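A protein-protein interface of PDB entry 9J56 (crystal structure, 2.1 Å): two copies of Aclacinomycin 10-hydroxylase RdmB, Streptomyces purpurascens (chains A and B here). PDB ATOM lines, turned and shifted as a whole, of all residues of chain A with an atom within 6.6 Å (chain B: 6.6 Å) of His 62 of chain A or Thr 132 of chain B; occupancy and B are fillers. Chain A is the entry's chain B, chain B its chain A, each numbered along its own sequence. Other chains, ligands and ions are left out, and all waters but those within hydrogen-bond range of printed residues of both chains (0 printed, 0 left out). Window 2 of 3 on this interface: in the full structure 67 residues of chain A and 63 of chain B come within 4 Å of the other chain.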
ATOM      1  N   LEU A  55      17.268   4.705 -20.668  1.00  0.00           N
ATOM      2  CA  LEU A  55      17.706   6.081 -20.514  1.00  0.00           C
ATOM      3  C   LEU A  55      16.579   7.037 -20.899  1.00  0.00           C
ATOM      4  O   LEU A  55      15.735   6.707 -21.741  1.00  0.00           O
ATOM      5  CB  LEU A  55      18.963   6.327 -21.361  1.00  0.00           C
ATOM      6  CG  LEU A  55      20.265   6.375 -20.550  1.00  0.00           C
ATOM      7  CD1 LEU A  55      20.692   4.979 -20.127  1.00  0.00           C
ATOM      8  CD2 LEU A  55      21.385   7.061 -21.324  1.00  0.00           C
ATOM      9  N   ASP A  60      13.414   9.871 -20.263  1.00  0.00           N
ATOM     10  CA  ASP A  60      12.212  10.422 -20.912  1.00  0.00           C
ATOM     11  C   ASP A  60      12.529  10.919 -22.337  1.00  0.00           C
ATOM     12  O   ASP A  60      11.978  11.910 -22.821  1.00  0.00           O
ATOM     13  CB  ASP A  60      11.584  11.521 -20.033  1.00  0.00           C
ATOM     14  CG  ASP A  60      10.455  12.272 -20.707  1.00  0.00           C
ATOM     15  OD1 ASP A  60       9.495  11.618 -21.169  1.00  0.00           O
ATOM     16  OD2 ASP A  60      10.536  13.519 -20.771  1.00  0.00           O
ATOM     17  N   THR A  61      13.412  10.213 -23.033  1.00  0.00           N
ATOM     18  CA  THR A  61      13.808  10.607 -24.377  1.00  0.00           C
ATOM     19  C   THR A  61      13.433   9.516 -25.369  1.00  0.00           C
ATOM     20  O   THR A  61      13.286   8.346 -25.004  1.00  0.00           O
ATOM     21  CB  THR A  61      15.310  10.876 -24.457  1.00  0.00           C
ATOM     22  OG1 THR A  61      16.015   9.824 -23.789  1.00  0.00           O
ATOM     23  CG2 THR A  61      15.643  12.185 -23.768  1.00  0.00           C
ATOM     24  N   HIS A  62      13.263   9.915 -26.619  1.00  0.00           N
ATOM     25  CA  HIS A  62      13.066   8.970 -27.722  1.00  0.00           C
ATOM     26  C   HIS A  62      14.362   8.200 -27.953  1.00  0.00           C
ATOM     27  O   HIS A  62      15.404   8.820 -28.210  1.00  0.00           O
ATOM     28  CB  HIS A  62      12.612   9.742 -28.963  1.00  0.00           C
ATOM     29  CG  HIS A  62      12.535   8.929 -30.216  1.00  0.00           C
ATOM     30  ND1 HIS A  62      13.648   8.400 -30.837  1.00  0.00           N
ATOM     31  CD2 HIS A  62      11.475   8.564 -30.976  1.00  0.00           C
ATOM     32  CE1 HIS A  62      13.277   7.745 -31.921  1.00  0.00           C
ATOM     33  NE2 HIS A  62      11.964   7.831 -32.032  1.00  0.00           N
ATOM     34  N   PRO A  63      14.349   6.864 -27.878  1.00  0.00           N
ATOM     35  CA  PRO A  63      15.622   6.127 -27.779  1.00  0.00           C
ATOM     36  C   PRO A  63      16.488   6.200 -29.027  1.00  0.00           C
ATOM     37  O   PRO A  63      17.717   6.267 -28.903  1.00  0.00           O
ATOM     38  CB  PRO A  63      15.178   4.683 -27.479  1.00  0.00           C
ATOM     39  CG  PRO A  63      13.702   4.773 -27.119  1.00  0.00           C
ATOM     40  CD  PRO A  63      13.187   5.963 -27.865  1.00  0.00           C
ATOM     41  N   GLN A  64      15.907   6.178 -30.228  1.00  0.00           N
ATOM     42  CA  GLN A  64      16.754   6.304 -31.413  1.00  0.00           C
ATOM     43  C   GLN A  64      17.299   7.722 -31.531  1.00  0.00           C
ATOM     44  O   GLN A  64      18.462   7.916 -31.906  1.00  0.00           O
ATOM     45  CB  GLN A  64      15.987   5.890 -32.671  1.00  0.00           C
ATOM     46  CG  GLN A  64      16.471   4.576 -33.330  1.00  0.00           C
ATOM     47  CD  GLN A  64      17.622   4.760 -34.343  1.00  0.00           C
ATOM     48  OE1 GLN A  64      17.866   5.863 -34.827  1.00  0.00           O
ATOM     49  NE2 GLN A  64      18.300   3.660 -34.688  1.00  0.00           N
ATOM     50  N   ALA A  65      16.490   8.721 -31.167  1.00  0.00           N
ATOM     51  CA  ALA A  65      16.959  10.105 -31.194  1.00  0.00           C
ATOM     52  C   ALA A  65      18.033  10.346 -30.140  1.00  0.00           C
ATOM     53  O   ALA A  65      19.022  11.041 -30.401  1.00  0.00           O
ATOM     54  CB  ALA A  65      15.785  11.067 -31.001  1.00  0.00           C
ATOM     55  N   LEU A  66      17.866   9.774 -28.946  1.00  0.00           N
ATOM     56  CA  LEU A  66      18.903   9.901 -27.930  1.00  0.00           C
ATOM     57  C   LEU A  66      20.206   9.240 -28.374  1.00  0.00           C
ATOM     58  O   LEU A  66      21.293   9.760 -28.095  1.00  0.00           O
ATOM     59  CB  LEU A  66      18.422   9.318 -26.601  1.00  0.00           C
ATOM     60  CG  LEU A  66      19.405   9.574 -25.456  1.00  0.00           C
ATOM     61  CD1 LEU A  66      19.523  11.059 -25.138  1.00  0.00           C
ATOM     62  CD2 LEU A  66      19.040   8.763 -24.228  1.00  0.00           C
ATOM     63  N   SER A  67      20.128   8.098 -29.071  1.00  0.00           N
ATOM     64  CA  SER A  67      21.355   7.467 -29.557  1.00  0.00           C
ATOM     65  C   SER A  67      22.039   8.336 -30.606  1.00  0.00           C
ATOM     66  O   SER A  67      23.272   8.446 -30.621  1.00  0.00           O
ATOM     67  CB  SER A  67      21.069   6.080 -30.139  1.00  0.00           C
ATOM     68  OG  SER A  67      19.857   6.061 -30.875  1.00  0.00           O
ATOM     69  N   ARG A  68      21.253   8.977 -31.477  1.00  0.00           N
ATOM     70  CA  ARG A  68      21.830   9.862 -32.482  1.00  0.00           C
ATOM     71  C   ARG A  68      22.527  11.058 -31.844  1.00  0.00           C
ATOM     72  O   ARG A  68      23.562  11.506 -32.349  1.00  0.00           O
ATOM     73  CB  ARG A  68      20.744  10.304 -33.466  1.00  0.00           C
ATOM     74  CG  ARG A  68      20.245   9.143 -34.360  1.00  0.00           C
ATOM     75  CD  ARG A  68      18.867   9.391 -34.966  1.00  0.00           C
ATOM     76  NE  ARG A  68      18.947  10.290 -36.112  1.00  0.00           N
ATOM     77  CZ  ARG A  68      17.941  10.548 -36.935  1.00  0.00           C
ATOM     78  NH1 ARG A  68      16.748  10.002 -36.764  1.00  0.00           N
ATOM     79  NH2 ARG A  68      18.136  11.374 -37.954  1.00  0.00           N
ATOM     80  N   LEU B 127      15.972  20.040 -27.614  1.00  0.00           N
ATOM     81  CA  LEU B 127      15.515  19.255 -26.477  1.00  0.00           C
ATOM     82  C   LEU B 127      14.257  18.476 -26.825  1.00  0.00           C
ATOM     83  O   LEU B 127      14.158  17.277 -26.544  1.00  0.00           O
ATOM     84  CB  LEU B 127      15.277  20.165 -25.264  1.00  0.00           C
ATOM     85  CG  LEU B 127      14.966  19.380 -23.987  1.00  0.00           C
ATOM     86  CD1 LEU B 127      16.229  18.745 -23.432  1.00  0.00           C
ATOM     87  CD2 LEU B 127      14.311  20.292 -22.923  1.00  0.00           C
ATOM     88  N   ASP B 128      13.279  19.146 -27.442  1.00  0.00           N
ATOM     89  CA  ASP B 128      12.059  18.459 -27.855  1.00  0.00           C
ATOM     90  C   ASP B 128      12.359  17.373 -28.882  1.00  0.00           C
ATOM     91  O   ASP B 128      11.726  16.312 -28.873  1.00  0.00           O
ATOM     92  CB  ASP B 128      11.059  19.464 -28.424  1.00  0.00           C
ATOM     93  N   VAL B 129      13.323  17.626 -29.780  1.00  0.00           N
ATOM     94  CA  VAL B 129      13.691  16.643 -30.803  1.00  0.00           C
ATOM     95  C   VAL B 129      14.133  15.334 -30.155  1.00  0.00           C
ATOM     96  O   VAL B 129      13.698  14.246 -30.553  1.00  0.00           O
ATOM     97  CB  VAL B 129      14.791  17.208 -31.721  1.00  0.00           C
ATOM     98  CG1 VAL B 129      15.413  16.087 -32.560  1.00  0.00           C
ATOM     99  CG2 VAL B 129      14.234  18.299 -32.626  1.00  0.00           C
ATOM    100  N   VAL B 130      15.016  15.423 -29.156  1.00  0.00           N
ATOM    101  CA  VAL B 130      15.500  14.237 -28.454  1.00  0.00           C
ATOM    102  C   VAL B 130      14.396  13.598 -27.614  1.00  0.00           C
ATOM    103  O   VAL B 130      14.420  12.384 -27.362  1.00  0.00           O
ATOM    104  CB  VAL B 130      16.726  14.605 -27.595  1.00  0.00           C
ATOM    105  CG1 VAL B 130      17.338  13.368 -26.974  1.00  0.00           C
ATOM    106  CG2 VAL B 130      17.762  15.305 -28.451  1.00  0.00           C
ATOM    107  N   ARG B 131      13.411  14.385 -27.170  1.00  0.00           N
ATOM    108  CA  ARG B 131      12.301  13.811 -26.416  1.00  0.00           C
ATOM    109  C   ARG B 131      11.312  13.077 -27.312  1.00  0.00           C
ATOM    110  O   ARG B 131      10.770  12.044 -26.913  1.00  0.00           O
ATOM    111  CB  ARG B 131      11.573  14.903 -25.636  1.00  0.00           C
ATOM    112  CG  ARG B 131      12.291  15.328 -24.392  1.00  0.00           C
ATOM    113  CD  ARG B 131      11.324  15.499 -23.236  1.00  0.00           C
ATOM    114  NE  ARG B 131      12.035  15.943 -22.047  1.00  0.00           N
ATOM    115  CZ  ARG B 131      12.267  17.217 -21.768  1.00  0.00           C
ATOM    116  NH1 ARG B 131      11.903  18.178 -22.605  1.00  0.00           N
ATOM    117  NH2 ARG B 131      12.866  17.536 -20.619  1.00  0.00           N
ATOM    118  N   THR B 132      11.066  13.583 -28.523  1.00  0.00           N
ATOM    119  CA  THR B 132       9.945  13.117 -29.326  1.00  0.00           C
ATOM    120  C   THR B 132      10.333  12.468 -30.649  1.00  0.00           C
ATOM    121  O   THR B 132       9.487  11.792 -31.245  1.00  0.00           O
ATOM    122  CB  THR B 132       8.990  14.280 -29.638  1.00  0.00           C
ATOM    123  OG1 THR B 132       9.649  15.197 -30.522  1.00  0.00           O
ATOM    124  CG2 THR B 132       8.578  15.016 -28.366  1.00  0.00           C
ATOM    125  N   GLY B 133      11.559  12.672 -31.139  1.00  0.00           N
ATOM    126  CA  GLY B 133      11.928  12.219 -32.462  1.00  0.00           C
ATOM    127  C   GLY B 133      11.368  13.052 -33.591  1.00  0.00           C
ATOM    128  O   GLY B 133      11.597  12.717 -34.762  1.00  0.00           O
ATOM    129  N   ARG B 134      10.639  14.160 -33.278  1.00  0.00           N
ATOM    130  CA  ARG B 134      10.038  14.973 -34.321  1.00  0.00           C
ATOM    131  C   ARG B 134      10.877  16.215 -34.587  1.00  0.00           C
ATOM    132  O   ARG B 134      11.581  16.702 -33.699  1.00  0.00           O
ATOM    133  CB  ARG B 134       8.611  15.378 -33.937  1.00  0.00           C
ATOM    134  CG  ARG B 134       7.679  14.198 -33.639  1.00  0.00           C
ATOM    135  CD  ARG B 134       6.200  14.659 -33.568  1.00  0.00           C
ATOM    136  N   PRO B 135      10.853  16.721 -35.817  1.00  0.00           N
ATOM    137  CA  PRO B 135      11.680  17.883 -36.152  1.00  0.00           C
ATOM    138  C   PRO B 135      11.228  19.142 -35.420  1.00  0.00           C
ATOM    139  O   PRO B 135      10.085  19.268 -34.966  1.00  0.00           O
ATOM    140  CB  PRO B 135      11.498  18.021 -37.670  1.00  0.00           C
ATOM    141  CG  PRO B 135      10.279  17.213 -37.995  1.00  0.00           C
ATOM    142  CD  PRO B 135      10.271  16.098 -37.019  1.00  0.00           C
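The backbone NH (N) of His 62 of chain A lies within hydrogen-bond range of the backbone carbonyl oxygen (O) of Val 130 of chain B, at 2.8 Å. The guanidinium group (NE) of Arg 131 of chain B lies within salt-bridge range of the side-chain carboxylate (OD2) of Asp 60 of chain A, at 3.1 Å. The backbone carbonyl oxygen of Arg 131 of chain B is in hydrogen-bond range of the backbone NH of His 62 of chain A (3.3 Å).
The backbone carbonyl oxygen (O) of Asp 128 of chain B sits at hydrogen-bond distance from the side-chain hydroxyl (OG1) of Thr 132 of chain B, at 2.9 Å. OG1 of Thr 132 of chain B lies within hydrogen-bond range of N of Arg 134 of chain B (3.1 Å). The backbone NH (N) of Gln 64 of chain A sits at hydrogen-bond distance from a ring nitrogen (ND1) of His 62 of chain A (3.2 Å). A ring nitrogen (ND1) of His 62 of chain A sits at hydrogen-bond distance from the backbone NH of Ala 65 of chain A, 2.9 Å away.
Among the printed residues, merely in contact across the chains: Thr 61 of chain A with Val 130 of chain B, Thr 61 of chain A with Arg 131 of chain B, His 62 of chain A with Thr 132 of chain B, His 62 of chain A with Gly 133 of chain B, Ala 65 of chain A with Val 129 of chain B and Leu 66 of chain A with Val 130 of chain B.
His 62 of chain A touches just these residues of chain B: Val 130 (2.8 Å), Arg 131 (3.3 Å), Thr 132 (3.8 Å) and Gly 133 (3.8 Å). Of chain A, only His 62 (3.8 Å) comes within 4 Å of Thr 132 of chain B. Of the printed residues of chain A, Arg 131 of chain B touches Asp 60, Thr 61 and His 62. Printed residues of chain A within 4 Å of Val 129 of chain B: Ala 65 (3.8 Å). Of the printed residues of chain B, Leu 66 of chain A touches Val 130. Of the printed residues of chain A, Val 130 of chain B touches Thr 61, His 62 and Leu 66. Of the printed residues of chain A, Gly 133 of chain B touches His 62. The nearest residue of chain B that does not touch His 62 of chain A is Val 129 of chain B (4.9 Å). The nearest printed residue of chain A that does not touch Thr 132 of chain B is Ala 65 of chain A (5.6 Å).
Of the 10 printed residues of chain A, 5 touch a printed residue of chain B. Hydrophobic or aromatic side chains of chain A within 4 Å of the printed part of chain B: His 62, Ala 65 and Leu 66. Along chain A the printed residues that touch a printed residue of chain B span positions 60 to 66. Of the 9 printed residues of chain B, 5 touch a printed residue of chain A. Along chain B the printed residues that touch a printed residue of chain A span positions 129 to 133. Among the printed residues, Asp or Glu carboxylates within 4 Å of a Lys or Arg side-chain nitrogen of the other chain: Asp 60 of chain A with Arg 131 of chain B.
No position is printed for both chains. Of the 9 pairs that touch across the chains among the printed residues, none has its exchanged pair printed and touching as well.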
